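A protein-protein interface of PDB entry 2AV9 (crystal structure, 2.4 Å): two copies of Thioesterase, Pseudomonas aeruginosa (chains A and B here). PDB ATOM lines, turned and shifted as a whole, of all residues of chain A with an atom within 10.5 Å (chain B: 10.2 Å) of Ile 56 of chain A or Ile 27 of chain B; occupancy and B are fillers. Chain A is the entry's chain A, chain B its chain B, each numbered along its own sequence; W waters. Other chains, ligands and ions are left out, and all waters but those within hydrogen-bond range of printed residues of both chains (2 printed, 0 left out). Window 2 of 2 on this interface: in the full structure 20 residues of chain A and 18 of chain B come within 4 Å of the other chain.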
ATOM      1  N   ASP A  41     -31.198  12.858  11.073  1.00  0.00           N
ATOM      2  CA  ASP A  41     -29.823  13.293  10.811  1.00  0.00           C
ATOM      3  C   ASP A  41     -29.353  14.391  11.766  1.00  0.00           C
ATOM      4  O   ASP A  41     -28.216  14.367  12.251  1.00  0.00           O
ATOM      5  CB  ASP A  41     -29.731  13.925   9.419  1.00  0.00           C
ATOM      6  CG  ASP A  41     -29.073  13.039   8.378  1.00  0.00           C
ATOM      7  OD1 ASP A  41     -28.510  11.980   8.738  1.00  0.00           O
ATOM      8  OD2 ASP A  41     -29.120  13.424   7.190  1.00  0.00           O
ATOM      9  N   THR A  42     -30.241  15.355  11.993  1.00  0.00           N
ATOM     10  CA  THR A  42     -29.954  16.472  12.881  1.00  0.00           C
ATOM     11  C   THR A  42     -29.792  16.028  14.332  1.00  0.00           C
ATOM     12  O   THR A  42     -28.836  16.443  14.980  1.00  0.00           O
ATOM     13  CB  THR A  42     -31.050  17.569  12.782  1.00  0.00           C
ATOM     14  OG1 THR A  42     -30.977  18.129  11.458  1.00  0.00           O
ATOM     15  CG2 THR A  42     -30.849  18.622  13.875  1.00  0.00           C
ATOM     16  N   VAL A  44     -29.201  13.022  15.622  1.00  0.00           N
ATOM     17  CA  VAL A  44     -28.073  12.123  15.841  1.00  0.00           C
ATOM     18  C   VAL A  44     -26.736  12.842  15.749  1.00  0.00           C
ATOM     19  O   VAL A  44     -25.896  12.730  16.633  1.00  0.00           O
ATOM     20  CB  VAL A  44     -28.160  10.928  14.882  1.00  0.00           C
ATOM     21  CG1 VAL A  44     -26.813  10.210  14.833  1.00  0.00           C
ATOM     22  CG2 VAL A  44     -29.310   9.997  15.340  1.00  0.00           C
ATOM     23  N   ASN A  45     -26.549  13.646  14.711  1.00  0.00           N
ATOM     24  CA  ASN A  45     -25.258  14.318  14.604  1.00  0.00           C
ATOM     25  C   ASN A  45     -25.025  15.422  15.625  1.00  0.00           C
ATOM     26  O   ASN A  45     -23.906  15.653  16.066  1.00  0.00           O
ATOM     27  CB  ASN A  45     -24.900  14.693  13.168  1.00  0.00           C
ATOM     28  CG  ASN A  45     -24.691  13.453  12.320  1.00  0.00           C
ATOM     29  OD1 ASN A  45     -23.645  12.824  12.403  1.00  0.00           O
ATOM     30  ND2 ASN A  45     -25.658  13.100  11.489  1.00  0.00           N
ATOM     31  N   THR A  46     -26.091  16.087  16.049  1.00  0.00           N
ATOM     32  CA  THR A  46     -25.923  17.030  17.161  1.00  0.00           C
ATOM     33  C   THR A  46     -25.366  16.331  18.387  1.00  0.00           C
ATOM     34  O   THR A  46     -24.385  16.750  18.966  1.00  0.00           O
ATOM     35  CB  THR A  46     -27.260  17.762  17.458  1.00  0.00           C
ATOM     36  OG1 THR A  46     -27.621  18.372  16.222  1.00  0.00           O
ATOM     37  CG2 THR A  46     -27.140  18.909  18.486  1.00  0.00           C
ATOM     38  N   TYR A  47     -25.979  15.220  18.768  1.00  0.00           N
ATOM     39  CA  TYR A  47     -25.500  14.405  19.873  1.00  0.00           C
ATOM     40  C   TYR A  47     -24.066  13.926  19.659  1.00  0.00           C
ATOM     41  O   TYR A  47     -23.226  14.020  20.553  1.00  0.00           O
ATOM     42  CB  TYR A  47     -26.507  13.267  20.127  1.00  0.00           C
ATOM     43  CG  TYR A  47     -26.071  12.385  21.271  1.00  0.00           C
ATOM     44  CD1 TYR A  47     -26.349  12.749  22.574  1.00  0.00           C
ATOM     45  CD2 TYR A  47     -25.350  11.208  21.066  1.00  0.00           C
ATOM     46  CE1 TYR A  47     -25.954  11.950  23.626  1.00  0.00           C
ATOM     47  CE2 TYR A  47     -24.919  10.419  22.108  1.00  0.00           C
ATOM     48  CZ  TYR A  47     -25.237  10.796  23.404  1.00  0.00           C
ATOM     49  OH  TYR A  47     -24.871  10.084  24.534  1.00  0.00           O
ATOM     50  N   LEU A  48     -23.733  13.379  18.491  1.00  0.00           N
ATOM     51  CA  LEU A  48     -22.353  12.931  18.291  1.00  0.00           C
ATOM     52  C   LEU A  48     -21.335  14.064  18.417  1.00  0.00           C
ATOM     53  O   LEU A  48     -20.232  13.826  18.908  1.00  0.00           O
ATOM     54  CB  LEU A  48     -22.179  12.184  16.968  1.00  0.00           C
ATOM     55  CG  LEU A  48     -22.954  10.894  16.682  1.00  0.00           C
ATOM     56  CD1 LEU A  48     -22.532  10.478  15.253  1.00  0.00           C
ATOM     57  CD2 LEU A  48     -22.601   9.759  17.643  1.00  0.00           C
ATOM     58  N   ILE A  49     -21.670  15.280  17.994  1.00  0.00           N
ATOM     59  CA  ILE A  49     -20.713  16.382  18.030  1.00  0.00           C
ATOM     60  C   ILE A  49     -20.635  16.880  19.476  1.00  0.00           C
ATOM     61  O   ILE A  49     -19.555  17.091  19.996  1.00  0.00           O
ATOM     62  CB  ILE A  49     -21.110  17.577  17.116  1.00  0.00           C
ATOM     63  CG1 ILE A  49     -21.090  17.165  15.641  1.00  0.00           C
ATOM     64  CG2 ILE A  49     -20.245  18.806  17.440  1.00  0.00           C
ATOM     65  CD1 ILE A  49     -21.927  18.036  14.739  1.00  0.00           C
ATOM     66  N   GLU A  50     -21.767  17.079  20.148  1.00  0.00           N
ATOM     67  CA  GLU A  50     -21.796  17.669  21.489  1.00  0.00           C
ATOM     68  C   GLU A  50     -21.341  16.721  22.581  1.00  0.00           C
ATOM     69  O   GLU A  50     -20.605  17.114  23.474  1.00  0.00           O
ATOM     70  CB  GLU A  50     -23.215  18.123  21.840  1.00  0.00           C
ATOM     71  CG  GLU A  50     -23.605  19.443  21.196  1.00  0.00           C
ATOM     72  CD  GLU A  50     -25.054  19.844  21.459  1.00  0.00           C
ATOM     73  OE1 GLU A  50     -25.771  19.119  22.192  1.00  0.00           O
ATOM     74  OE2 GLU A  50     -25.457  20.881  20.883  1.00  0.00           O
ATOM     75  N   GLY A  52     -20.130  13.273  21.835  1.00  0.00           N
ATOM     76  CA  GLY A  52     -19.169  12.299  21.350  1.00  0.00           C
ATOM     77  C   GLY A  52     -17.888  12.937  20.844  1.00  0.00           C
ATOM     78  O   GLY A  52     -16.935  12.234  20.548  1.00  0.00           O
ATOM     79  N   GLY A  53     -17.843  14.261  20.726  1.00  0.00           N
ATOM     80  CA  GLY A  53     -16.689  14.928  20.136  1.00  0.00           C
ATOM     81  C   GLY A  53     -16.505  14.690  18.646  1.00  0.00           C
ATOM     82  O   GLY A  53     -15.434  14.993  18.125  1.00  0.00           O
ATOM     83  N   LEU A  54     -17.506  14.173  17.932  1.00  0.00           N
ATOM     84  CA  LEU A  54     -17.404  14.155  16.473  1.00  0.00           C
ATOM     85  C   LEU A  54     -16.965  15.509  15.902  1.00  0.00           C
ATOM     86  O   LEU A  54     -17.493  16.553  16.277  1.00  0.00           O
ATOM     87  CB  LEU A  54     -18.725  13.711  15.838  1.00  0.00           C
ATOM     88  CG  LEU A  54     -18.865  13.553  14.319  1.00  0.00           C
ATOM     89  CD1 LEU A  54     -18.012  12.441  13.710  1.00  0.00           C
ATOM     90  CD2 LEU A  54     -20.325  13.407  13.932  1.00  0.00           C
ATOM     91  N   ASP A  55     -15.997  15.478  14.993  1.00  0.00           N
ATOM     92  CA  ASP A  55     -15.420  16.637  14.318  1.00  0.00           C
ATOM     93  C   ASP A  55     -15.759  16.537  12.839  1.00  0.00           C
ATOM     94  O   ASP A  55     -15.114  15.805  12.089  1.00  0.00           O
ATOM     95  CB  ASP A  55     -13.912  16.699  14.544  1.00  0.00           C
ATOM     96  CG  ASP A  55     -13.236  17.811  13.758  1.00  0.00           C
ATOM     97  OD1 ASP A  55     -13.933  18.696  13.231  1.00  0.00           O
ATOM     98  OD2 ASP A  55     -11.986  17.843  13.679  1.00  0.00           O
ATOM     99  N   ILE A  56     -16.801  17.255  12.429  1.00  0.00           N
ATOM    100  CA  ILE A  56     -17.372  17.102  11.097  1.00  0.00           C
ATOM    101  C   ILE A  56     -16.620  17.917  10.055  1.00  0.00           C
ATOM    102  O   ILE A  56     -16.773  17.674   8.858  1.00  0.00           O
ATOM    103  CB  ILE A  56     -18.897  17.415  11.034  1.00  0.00           C
ATOM    104  CG1 ILE A  56     -19.126  18.906  11.302  1.00  0.00           C
ATOM    105  CG2 ILE A  56     -19.733  16.334  11.827  1.00  0.00           C
ATOM    106  CD1 ILE A  56     -20.563  19.370  11.218  1.00  0.00           C
ATOM    107  N   GLN A  57     -15.822  18.871  10.519  1.00  0.00           N
ATOM    108  CA  GLN A  57     -15.037  19.734   9.665  1.00  0.00           C
ATOM    109  C   GLN A  57     -13.726  19.040   9.298  1.00  0.00           C
ATOM    110  O   GLN A  57     -13.370  19.025   8.118  1.00  0.00           O
ATOM    111  CB  GLN A  57     -14.744  21.078  10.351  1.00  0.00           C
ATOM    112  CG  GLN A  57     -15.941  21.865  10.897  1.00  0.00           C
ATOM    113  CD  GLN A  57     -16.848  22.419   9.800  1.00  0.00           C
ATOM    114  OE1 GLN A  57     -16.380  22.628   8.681  1.00  0.00           O
ATOM    115  NE2 GLN A  57     -18.137  22.632  10.094  1.00  0.00           N
ATOM    116  N   GLY A  58     -13.012  18.478  10.274  1.00  0.00           N
ATOM    117  CA  GLY A  58     -11.696  17.900  10.014  1.00  0.00           C
ATOM    118  C   GLY A  58     -11.493  16.561  10.704  1.00  0.00           C
ATOM    119  O   GLY A  58     -10.383  16.042  10.768  1.00  0.00           O
ATOM    120  N   GLY A  59     -12.551  15.960  11.240  1.00  0.00           N
ATOM    121  CA  GLY A  59     -12.333  14.670  11.876  1.00  0.00           C
ATOM    122  C   GLY A  59     -11.904  13.579  10.911  1.00  0.00           C
ATOM    123  O   GLY A  59     -12.189  13.617   9.715  1.00  0.00           O
ATOM    124  N   GLU A  60     -11.214  12.576  11.439  1.00  0.00           N
ATOM    125  CA  GLU A  60     -10.733  11.482  10.606  1.00  0.00           C
ATOM    126  C   GLU A  60     -11.760  10.362  10.450  1.00  0.00           C
ATOM    127  O   GLU A  60     -11.715   9.603   9.488  1.00  0.00           O
ATOM    128  CB  GLU A  60      -9.426  10.924  11.158  1.00  0.00           C
ATOM    129  CG  GLU A  60      -8.186  11.660  10.643  1.00  0.00           C
ATOM    130  N   VAL A  61     -12.684  10.246  11.398  1.00  0.00           N
ATOM    131  CA  VAL A  61     -13.663   9.176  11.375  1.00  0.00           C
ATOM    132  C   VAL A  61     -15.023   9.847  11.274  1.00  0.00           C
ATOM    133  O   VAL A  61     -15.273  10.775  12.034  1.00  0.00           O
ATOM    134  CB  VAL A  61     -13.575   8.279  12.636  1.00  0.00           C
ATOM    135  CG1 VAL A  61     -14.662   7.240  12.616  1.00  0.00           C
ATOM    136  CG2 VAL A  61     -12.248   7.553  12.705  1.00  0.00           C
ATOM    137  N   ILE A  62     -15.871   9.398  10.351  1.00  0.00           N
ATOM    138  CA  ILE A  62     -17.237   9.909  10.223  1.00  0.00           C
ATOM    139  C   ILE A  62     -18.274   8.781  10.212  1.00  0.00           C
ATOM    140  O   ILE A  62     -17.960   7.599   9.993  1.00  0.00           O
ATOM    141  CB  ILE A  62     -17.348  10.780   8.978  1.00  0.00           C
ATOM    142  CG1 ILE A  62     -16.959   9.986   7.734  1.00  0.00           C
ATOM    143  CG2 ILE A  62     -16.324  11.913   9.086  1.00  0.00           C
ATOM    144  CD1 ILE A  62     -17.253  10.586   6.356  1.00  0.00           C
ATOM    145  N   GLY A  63     -19.528   9.135  10.495  1.00  0.00           N
ATOM    146  CA  GLY A  63     -20.598   8.150  10.399  1.00  0.00           C
ATOM    147  C   GLY A  63     -21.348   8.346   9.101  1.00  0.00           C
ATOM    148  O   GLY A  63     -21.713   9.477   8.795  1.00  0.00           O
ATOM    149  N   LEU A  64     -21.565   7.259   8.371  1.00  0.00           N
ATOM    150  CA  LEU A  64     -22.341   7.258   7.137  1.00  0.00           C
ATOM    151  C   LEU A  64     -23.568   6.398   7.384  1.00  0.00           C
ATOM    152  O   LEU A  64     -23.525   5.415   8.148  1.00  0.00           O
ATOM    153  CB  LEU A  64     -21.482   6.636   6.030  1.00  0.00           C
ATOM    154  CG  LEU A  64     -20.259   7.497   5.681  1.00  0.00           C
ATOM    155  CD1 LEU A  64     -19.640   7.061   4.372  1.00  0.00           C
ATOM    156  CD2 LEU A  64     -20.513   8.995   5.642  1.00  0.00           C
ATOM    157  N   HIS A 118     -25.676   3.950  11.435  1.00  0.00           N
ATOM    158  CA  HIS A 118     -24.421   4.554  11.002  1.00  0.00           C
ATOM    159  C   HIS A 118     -23.388   3.458  10.957  1.00  0.00           C
ATOM    160  O   HIS A 118     -23.362   2.596  11.840  1.00  0.00           O
ATOM    161  CB  HIS A 118     -23.887   5.557  12.026  1.00  0.00           C
ATOM    162  CG  HIS A 118     -24.235   6.980  11.734  1.00  0.00           C
ATOM    163  ND1 HIS A 118     -24.054   7.984  12.663  1.00  0.00           N
ATOM    164  CD2 HIS A 118     -24.762   7.574  10.638  1.00  0.00           C
ATOM    165  CE1 HIS A 118     -24.465   9.133  12.156  1.00  0.00           C
ATOM    166  NE2 HIS A 118     -24.889   8.916  10.923  1.00  0.00           N
ATOM    167  N   PHE A 120     -19.277   3.733  10.944  1.00  0.00           N
ATOM    168  CA  PHE A 120     -18.153   4.647  11.062  1.00  0.00           C
ATOM    169  C   PHE A 120     -16.980   4.223  10.194  1.00  0.00           C
ATOM    170  O   PHE A 120     -16.613   3.052  10.151  1.00  0.00           O
ATOM    171  CB  PHE A 120     -17.761   4.849  12.528  1.00  0.00           C
ATOM    172  CG  PHE A 120     -18.882   5.428  13.341  1.00  0.00           C
ATOM    173  CD1 PHE A 120     -19.822   4.602  13.922  1.00  0.00           C
ATOM    174  CD2 PHE A 120     -19.021   6.792  13.498  1.00  0.00           C
ATOM    175  CE1 PHE A 120     -20.878   5.088  14.683  1.00  0.00           C
ATOM    176  CE2 PHE A 120     -20.090   7.300  14.230  1.00  0.00           C
ATOM    177  CZ  PHE A 120     -20.999   6.456  14.831  1.00  0.00           C
ATOM    178  N   ARG A 123     -12.611   8.798   6.923  1.00  0.00           N
ATOM    179  CA  ARG A 123     -13.203   9.723   5.985  1.00  0.00           C
ATOM    180  C   ARG A 123     -12.556   9.704   4.605  1.00  0.00           C
ATOM    181  O   ARG A 123     -13.239   9.953   3.605  1.00  0.00           O
ATOM    182  CB  ARG A 123     -13.047  11.107   6.592  1.00  0.00           C
ATOM    183  CG  ARG A 123     -13.750  12.224   5.885  1.00  0.00           C
ATOM    184  CD  ARG A 123     -13.282  13.467   6.625  1.00  0.00           C
ATOM    185  NE  ARG A 123     -14.131  14.623   6.364  1.00  0.00           N
ATOM    186  CZ  ARG A 123     -14.710  15.362   7.304  1.00  0.00           C
ATOM    187  NH1 ARG A 123     -14.556  15.082   8.596  1.00  0.00           N
ATOM    188  NH2 ARG A 123     -15.447  16.391   6.910  1.00  0.00           N
ATOM    189  N   LEU A 135     -16.533   8.200  21.024  1.00  0.00           N
ATOM    190  CA  LEU A 135     -17.838   8.034  20.392  1.00  0.00           C
ATOM    191  C   LEU A 135     -18.597   6.824  20.921  1.00  0.00           C
ATOM    192  O   LEU A 135     -19.794   6.976  21.161  1.00  0.00           O
ATOM    193  CB  LEU A 135     -17.814   7.998  18.858  1.00  0.00           C
ATOM    194  CG  LEU A 135     -17.380   9.218  18.041  1.00  0.00           C
ATOM    195  CD1 LEU A 135     -17.280   8.888  16.567  1.00  0.00           C
ATOM    196  CD2 LEU A 135     -18.395  10.341  18.211  1.00  0.00           C
ATOM    197  N   TRP B  22     -26.726  21.007  -6.970  1.00  0.00           N
ATOM    198  CA  TRP B  22     -25.505  21.314  -6.250  1.00  0.00           C
ATOM    199  C   TRP B  22     -25.575  21.057  -4.749  1.00  0.00           C
ATOM    200  O   TRP B  22     -24.648  20.456  -4.186  1.00  0.00           O
ATOM    201  CB  TRP B  22     -25.165  22.787  -6.478  1.00  0.00           C
ATOM    202  CG  TRP B  22     -24.092  23.335  -5.582  1.00  0.00           C
ATOM    203  CD1 TRP B  22     -24.225  24.292  -4.578  1.00  0.00           C
ATOM    204  CD2 TRP B  22     -22.702  22.982  -5.628  1.00  0.00           C
ATOM    205  NE1 TRP B  22     -22.991  24.528  -4.013  1.00  0.00           N
ATOM    206  CE2 TRP B  22     -22.047  23.753  -4.641  1.00  0.00           C
ATOM    207  CE3 TRP B  22     -21.965  22.076  -6.395  1.00  0.00           C
ATOM    208  CZ2 TRP B  22     -20.672  23.667  -4.417  1.00  0.00           C
ATOM    209  CZ3 TRP B  22     -20.596  21.979  -6.170  1.00  0.00           C
ATOM    210  CH2 TRP B  22     -19.969  22.766  -5.181  1.00  0.00           C
ATOM    211  N   HIS B  23     -26.655  21.519  -4.119  1.00  0.00           N
ATOM    212  CA  HIS B  23     -26.759  21.357  -2.674  1.00  0.00           C
ATOM    213  C   HIS B  23     -27.343  20.011  -2.256  1.00  0.00           C
ATOM    214  O   HIS B  23     -27.552  19.860  -1.047  1.00  0.00           O
ATOM    215  CB  HIS B  23     -27.425  22.561  -1.985  1.00  0.00           C
ATOM    216  CG  HIS B  23     -27.323  22.613  -0.484  1.00  0.00           C
ATOM    217  ND1 HIS B  23     -26.195  22.254   0.230  1.00  0.00           N
ATOM    218  CD2 HIS B  23     -28.226  23.024   0.445  1.00  0.00           C
ATOM    219  CE1 HIS B  23     -26.408  22.436   1.522  1.00  0.00           C
ATOM    220  NE2 HIS B  23     -27.642  22.881   1.681  1.00  0.00           N
ATOM    221  N   ASP B  24     -27.583  19.072  -3.176  1.00  0.00           N
ATOM    222  CA  ASP B  24     -27.871  17.690  -2.746  1.00  0.00           C
ATOM    223  C   ASP B  24     -26.682  17.184  -1.923  1.00  0.00           C
ATOM    224  O   ASP B  24     -26.852  16.343  -1.026  1.00  0.00           O
ATOM    225  CB  ASP B  24     -28.061  16.737  -3.932  1.00  0.00           C
ATOM    226  CG  ASP B  24     -29.354  16.991  -4.677  1.00  0.00           C
ATOM    227  OD1 ASP B  24     -30.235  17.639  -4.091  1.00  0.00           O
ATOM    228  OD2 ASP B  24     -29.529  16.533  -5.828  1.00  0.00           O
ATOM    229  N   ASN B  25     -25.477  17.671  -2.242  1.00  0.00           N
ATOM    230  CA  ASN B  25     -24.331  17.080  -1.560  1.00  0.00           C
ATOM    231  C   ASN B  25     -24.316  17.473  -0.095  1.00  0.00           C
ATOM    232  O   ASN B  25     -24.661  18.605   0.219  1.00  0.00           O
ATOM    233  CB  ASN B  25     -22.977  17.431  -2.146  1.00  0.00           C
ATOM    234  CG  ASN B  25     -22.726  16.701  -3.445  1.00  0.00           C
ATOM    235  OD1 ASN B  25     -23.312  15.650  -3.772  1.00  0.00           O
ATOM    236  ND2 ASN B  25     -21.824  17.290  -4.207  1.00  0.00           N
ATOM    237  N   ASP B  26     -23.983  16.582   0.836  1.00  0.00           N
ATOM    238  CA  ASP B  26     -23.749  17.190   2.143  1.00  0.00           C
ATOM    239  C   ASP B  26     -22.289  17.481   2.429  1.00  0.00           C
ATOM    240  O   ASP B  26     -21.454  17.390   1.540  1.00  0.00           O
ATOM    241  CB  ASP B  26     -24.430  16.460   3.308  1.00  0.00           C
ATOM    242  CG  ASP B  26     -23.838  15.080   3.569  1.00  0.00           C
ATOM    243  OD1 ASP B  26     -22.763  14.748   3.018  1.00  0.00           O
ATOM    244  OD2 ASP B  26     -24.476  14.294   4.318  1.00  0.00           O
ATOM    245  N   ILE B  27     -21.992  17.815   3.680  1.00  0.00           N
ATOM    246  CA  ILE B  27     -20.639  18.093   4.147  1.00  0.00           C
ATOM    247  C   ILE B  27     -19.591  17.044   3.806  1.00  0.00           C
ATOM    248  O   ILE B  27     -18.419  17.408   3.719  1.00  0.00           O
ATOM    249  CB  ILE B  27     -20.625  18.464   5.662  1.00  0.00           C
ATOM    250  CG1 ILE B  27     -19.408  19.322   6.019  1.00  0.00           C
ATOM    251  CG2 ILE B  27     -20.915  17.286   6.600  1.00  0.00           C
ATOM    252  CD1 ILE B  27     -19.324  19.767   7.468  1.00  0.00           C
ATOM    253  N   TYR B  28     -19.995  15.790   3.605  1.00  0.00           N
ATOM    254  CA  TYR B  28     -19.032  14.726   3.324  1.00  0.00           C
ATOM    255  C   TYR B  28     -18.878  14.576   1.816  1.00  0.00           C
ATOM    256  O   TYR B  28     -18.163  13.681   1.402  1.00  0.00           O
ATOM    257  CB  TYR B  28     -19.425  13.428   4.046  1.00  0.00           C
ATOM    258  CG  TYR B  28     -19.546  13.491   5.558  1.00  0.00           C
ATOM    259  CD1 TYR B  28     -18.669  14.244   6.336  1.00  0.00           C
ATOM    260  CD2 TYR B  28     -20.547  12.794   6.221  1.00  0.00           C
ATOM    261  CE1 TYR B  28     -18.799  14.284   7.711  1.00  0.00           C
ATOM    262  CE2 TYR B  28     -20.678  12.806   7.599  1.00  0.00           C
ATOM    263  CZ  TYR B  28     -19.794  13.558   8.340  1.00  0.00           C
ATOM    264  OH  TYR B  28     -19.947  13.552   9.712  1.00  0.00           O
ATOM    265  N   GLY B  29     -19.504  15.438   1.013  1.00  0.00           N
ATOM    266  CA  GLY B  29     -19.260  15.454  -0.443  1.00  0.00           C
ATOM    267  C   GLY B  29     -20.148  14.569  -1.303  1.00  0.00           C
ATOM    268  O   GLY B  29     -19.958  14.605  -2.508  1.00  0.00           O
ATOM    269  N   HIS B  30     -21.104  13.841  -0.729  1.00  0.00           N
ATOM    270  CA  HIS B  30     -22.016  12.902  -1.418  1.00  0.00           C
ATOM    271  C   HIS B  30     -23.463  13.248  -1.169  1.00  0.00           C
ATOM    272  O   HIS B  30     -23.731  13.971  -0.221  1.00  0.00           O
ATOM    273  CB  HIS B  30     -21.855  11.411  -1.064  1.00  0.00           C
ATOM    274  CG  HIS B  30     -20.505  10.906  -1.461  1.00  0.00           C
ATOM    275  ND1 HIS B  30     -20.134  10.786  -2.785  1.00  0.00           N
ATOM    276  CD2 HIS B  30     -19.396  10.639  -0.731  1.00  0.00           C
ATOM    277  CE1 HIS B  30     -18.875  10.393  -2.853  1.00  0.00           C
ATOM    278  NE2 HIS B  30     -18.406  10.307  -1.622  1.00  0.00           N
ATOM    279  N   VAL B  31     -24.348  12.731  -2.018  1.00  0.00           N
ATOM    280  CA  VAL B  31     -25.745  13.152  -1.966  1.00  0.00           C
ATOM    281  C   VAL B  31     -26.211  12.779  -0.564  1.00  0.00           C
ATOM    282  O   VAL B  31     -26.056  11.647  -0.128  1.00  0.00           O
ATOM    283  CB  VAL B  31     -26.595  12.507  -3.087  1.00  0.00           C
ATOM    284  CG1 VAL B  31     -28.070  12.519  -2.697  1.00  0.00           C
ATOM    285  CG2 VAL B  31     -26.378  13.263  -4.394  1.00  0.00           C
ATOM    286  N   ASN B  32     -26.775  13.719   0.176  1.00  0.00           N
ATOM    287  CA  ASN B  32     -27.300  13.402   1.507  1.00  0.00           C
ATOM    288  C   ASN B  32     -28.462  12.404   1.519  1.00  0.00           C
ATOM    289  O   ASN B  32     -29.194  12.257   0.538  1.00  0.00           O
ATOM    290  CB  ASN B  32     -27.718  14.657   2.272  1.00  0.00           C
ATOM    291  CG  ASN B  32     -28.322  14.314   3.638  1.00  0.00           C
ATOM    292  OD1 ASN B  32     -29.530  14.540   3.824  1.00  0.00           O
ATOM    293  ND2 ASN B  32     -27.524  13.742   4.562  1.00  0.00           N
ATOM    294  N   ASN B  33     -28.645  11.711   2.636  1.00  0.00           N
ATOM    295  CA  ASN B  33     -29.395  10.465   2.565  1.00  0.00           C
ATOM    296  C   ASN B  33     -30.871  10.818   2.581  1.00  0.00           C
ATOM    297  O   ASN B  33     -31.749  10.009   2.280  1.00  0.00           O
ATOM    298  CB  ASN B  33     -29.033   9.518   3.706  1.00  0.00           C
ATOM    299  CG  ASN B  33     -28.194  10.199   4.747  1.00  0.00           C
ATOM    300  OD1 ASN B  33     -28.711  10.741   5.729  1.00  0.00           O
ATOM    301  ND2 ASN B  33     -26.882  10.241   4.480  1.00  0.00           N
HETATM  302  O   HOH W   1     -30.070  15.847   6.581  1.00  0.00           O
HETATM  303  O   HOH W   2     -21.497  11.724  10.901  1.00  0.00           O
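Ile 56 of chain A touches Ile 27 of chain B (O to CD1, 3.6 Å). Ile 56 of chain A touches Tyr 28 of chain B (CG2 to OH, 3.5 Å). CG2 of Ile 62 of chain A touches CE1 of Tyr 28 of chain B (3.7 Å). O of Gly 63 of chain A touches CE2 of Tyr 28 of chain B (3.7 Å). Leu 64 of chain A touches Tyr 28 of chain B (CD2 to CD2, 3.8 Å). CD1 of Tyr 28 of chain B touches NH2 of Arg 123 of chain A, at 3.9 Å.
No position is printed for both chains. Of the 8 pairs that touch across the chains among the printed residues, none has its exchanged pair printed and touching as well.
The side-chain carboxylate (OD2) of Asp 41 of chain A is in hydrogen-bond range of the side-chain amide nitrogen (ND2) of Asn 32 of chain B (3.1 Å). OD2 of Asp 41 of chain A sits close to OD1 of Asn 33 of chain B, 3.1 Å away.
Of the printed residues of chain B, Ile 56 of chain A touches Ile 27 and Tyr 28. Ile 27 of chain B touches just one residue of chain A: Ile 56 (3.6 Å). No residue of chain B comes within 4 Å of Asp 55 of chain A. No residue of chain B comes within 4 Å of Gln 57 of chain A. Tyr 28 of chain B touches just these residues of chain A: Ile 56 (3.5 Å), Ile 62 (3.7 Å), Gly 63 (3.7 Å), Leu 64 (3.8 Å) and Arg 123 (3.9 Å). Of the printed residues of chain A, Asn 32 of chain B touches Asp 41 (3.1 Å). Printed residues of chain B within 4 Å of Leu 64 of chain A: Tyr 28. Val 61 of chain A touches none of the printed residues of chain B. The nearest residue of chain B that does not touch Ile 56 of chain A is Asp 26 of chain B (8.5 Å). The nearest residue of chain A that does not touch Ile 27 of chain B is Gln 57 of chain A (4.1 Å). The nearest printed residue of chain B that does not touch Asp 41 of chain A is Asp 26 of chain B (5.5 Å).
Of the 26 printed residues of chain A, 6 touch a printed residue of chain B. Hydrophobic or aromatic side chains of chain A that line the printed part of chain B: Ile 56, Ile 62 and Leu 64. Along chain A the printed residues that touch a printed residue of chain B span positions 41 to 123. Hydrophobic or aromatic side chains of chain B that line the printed part of chain A: Ile 27 and Tyr 28. Among the printed residues, 8 pairs touch across the chains. Among the printed residues, no Asp or Glu carboxylate lies within 4 Å of a Lys or Arg side-chain nitrogen of the other chain.
Water W1 lies within hydrogen-bond range of OD2 of Asp 41 of chain A (2.7 Å) and OD1 of Asn 32 of chain B (3.1 Å). Water W2 lies within hydrogen-bond range of the side-chain hydroxyl of Tyr 28 of chain B (2.7 Å), the side-chain amide oxygen of Asn 45 of chain A (2.8 Å) and the backbone carbonyl oxygen of Gly 63 of chain A (3.1 Å).
The backbone carbonyl oxygen (O) of Asp 41 of chain A is in hydrogen-bond range of the side-chain amide nitrogen (ND2) of Asn 45 of chain A. The backbone carbonyl oxygen of Ile 56 of chain A sits at hydrogen-bond distance from the guanidinium group of Arg 123 of chain A, at 2.7 Å. The backbone carbonyl oxygen (O) of Gly 59 of chain A is in hydrogen-bond range of the guanidinium group (NH1) of Arg 123 of chain A. O of Asp 24 of chain B lies within hydrogen-bond range of N of Asn 32 of chain B (2.9 Å). OD2 of Asp 26 of chain B lies within hydrogen-bond range of ND2 of Asn 32 of chain B (3.1 Å). The side-chain amide nitrogen (ND2) of Asn 32 of chain B sits at hydrogen-bond distance from the side-chain amide oxygen (OD1) of Asn 33 of chain B (3.4 Å).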
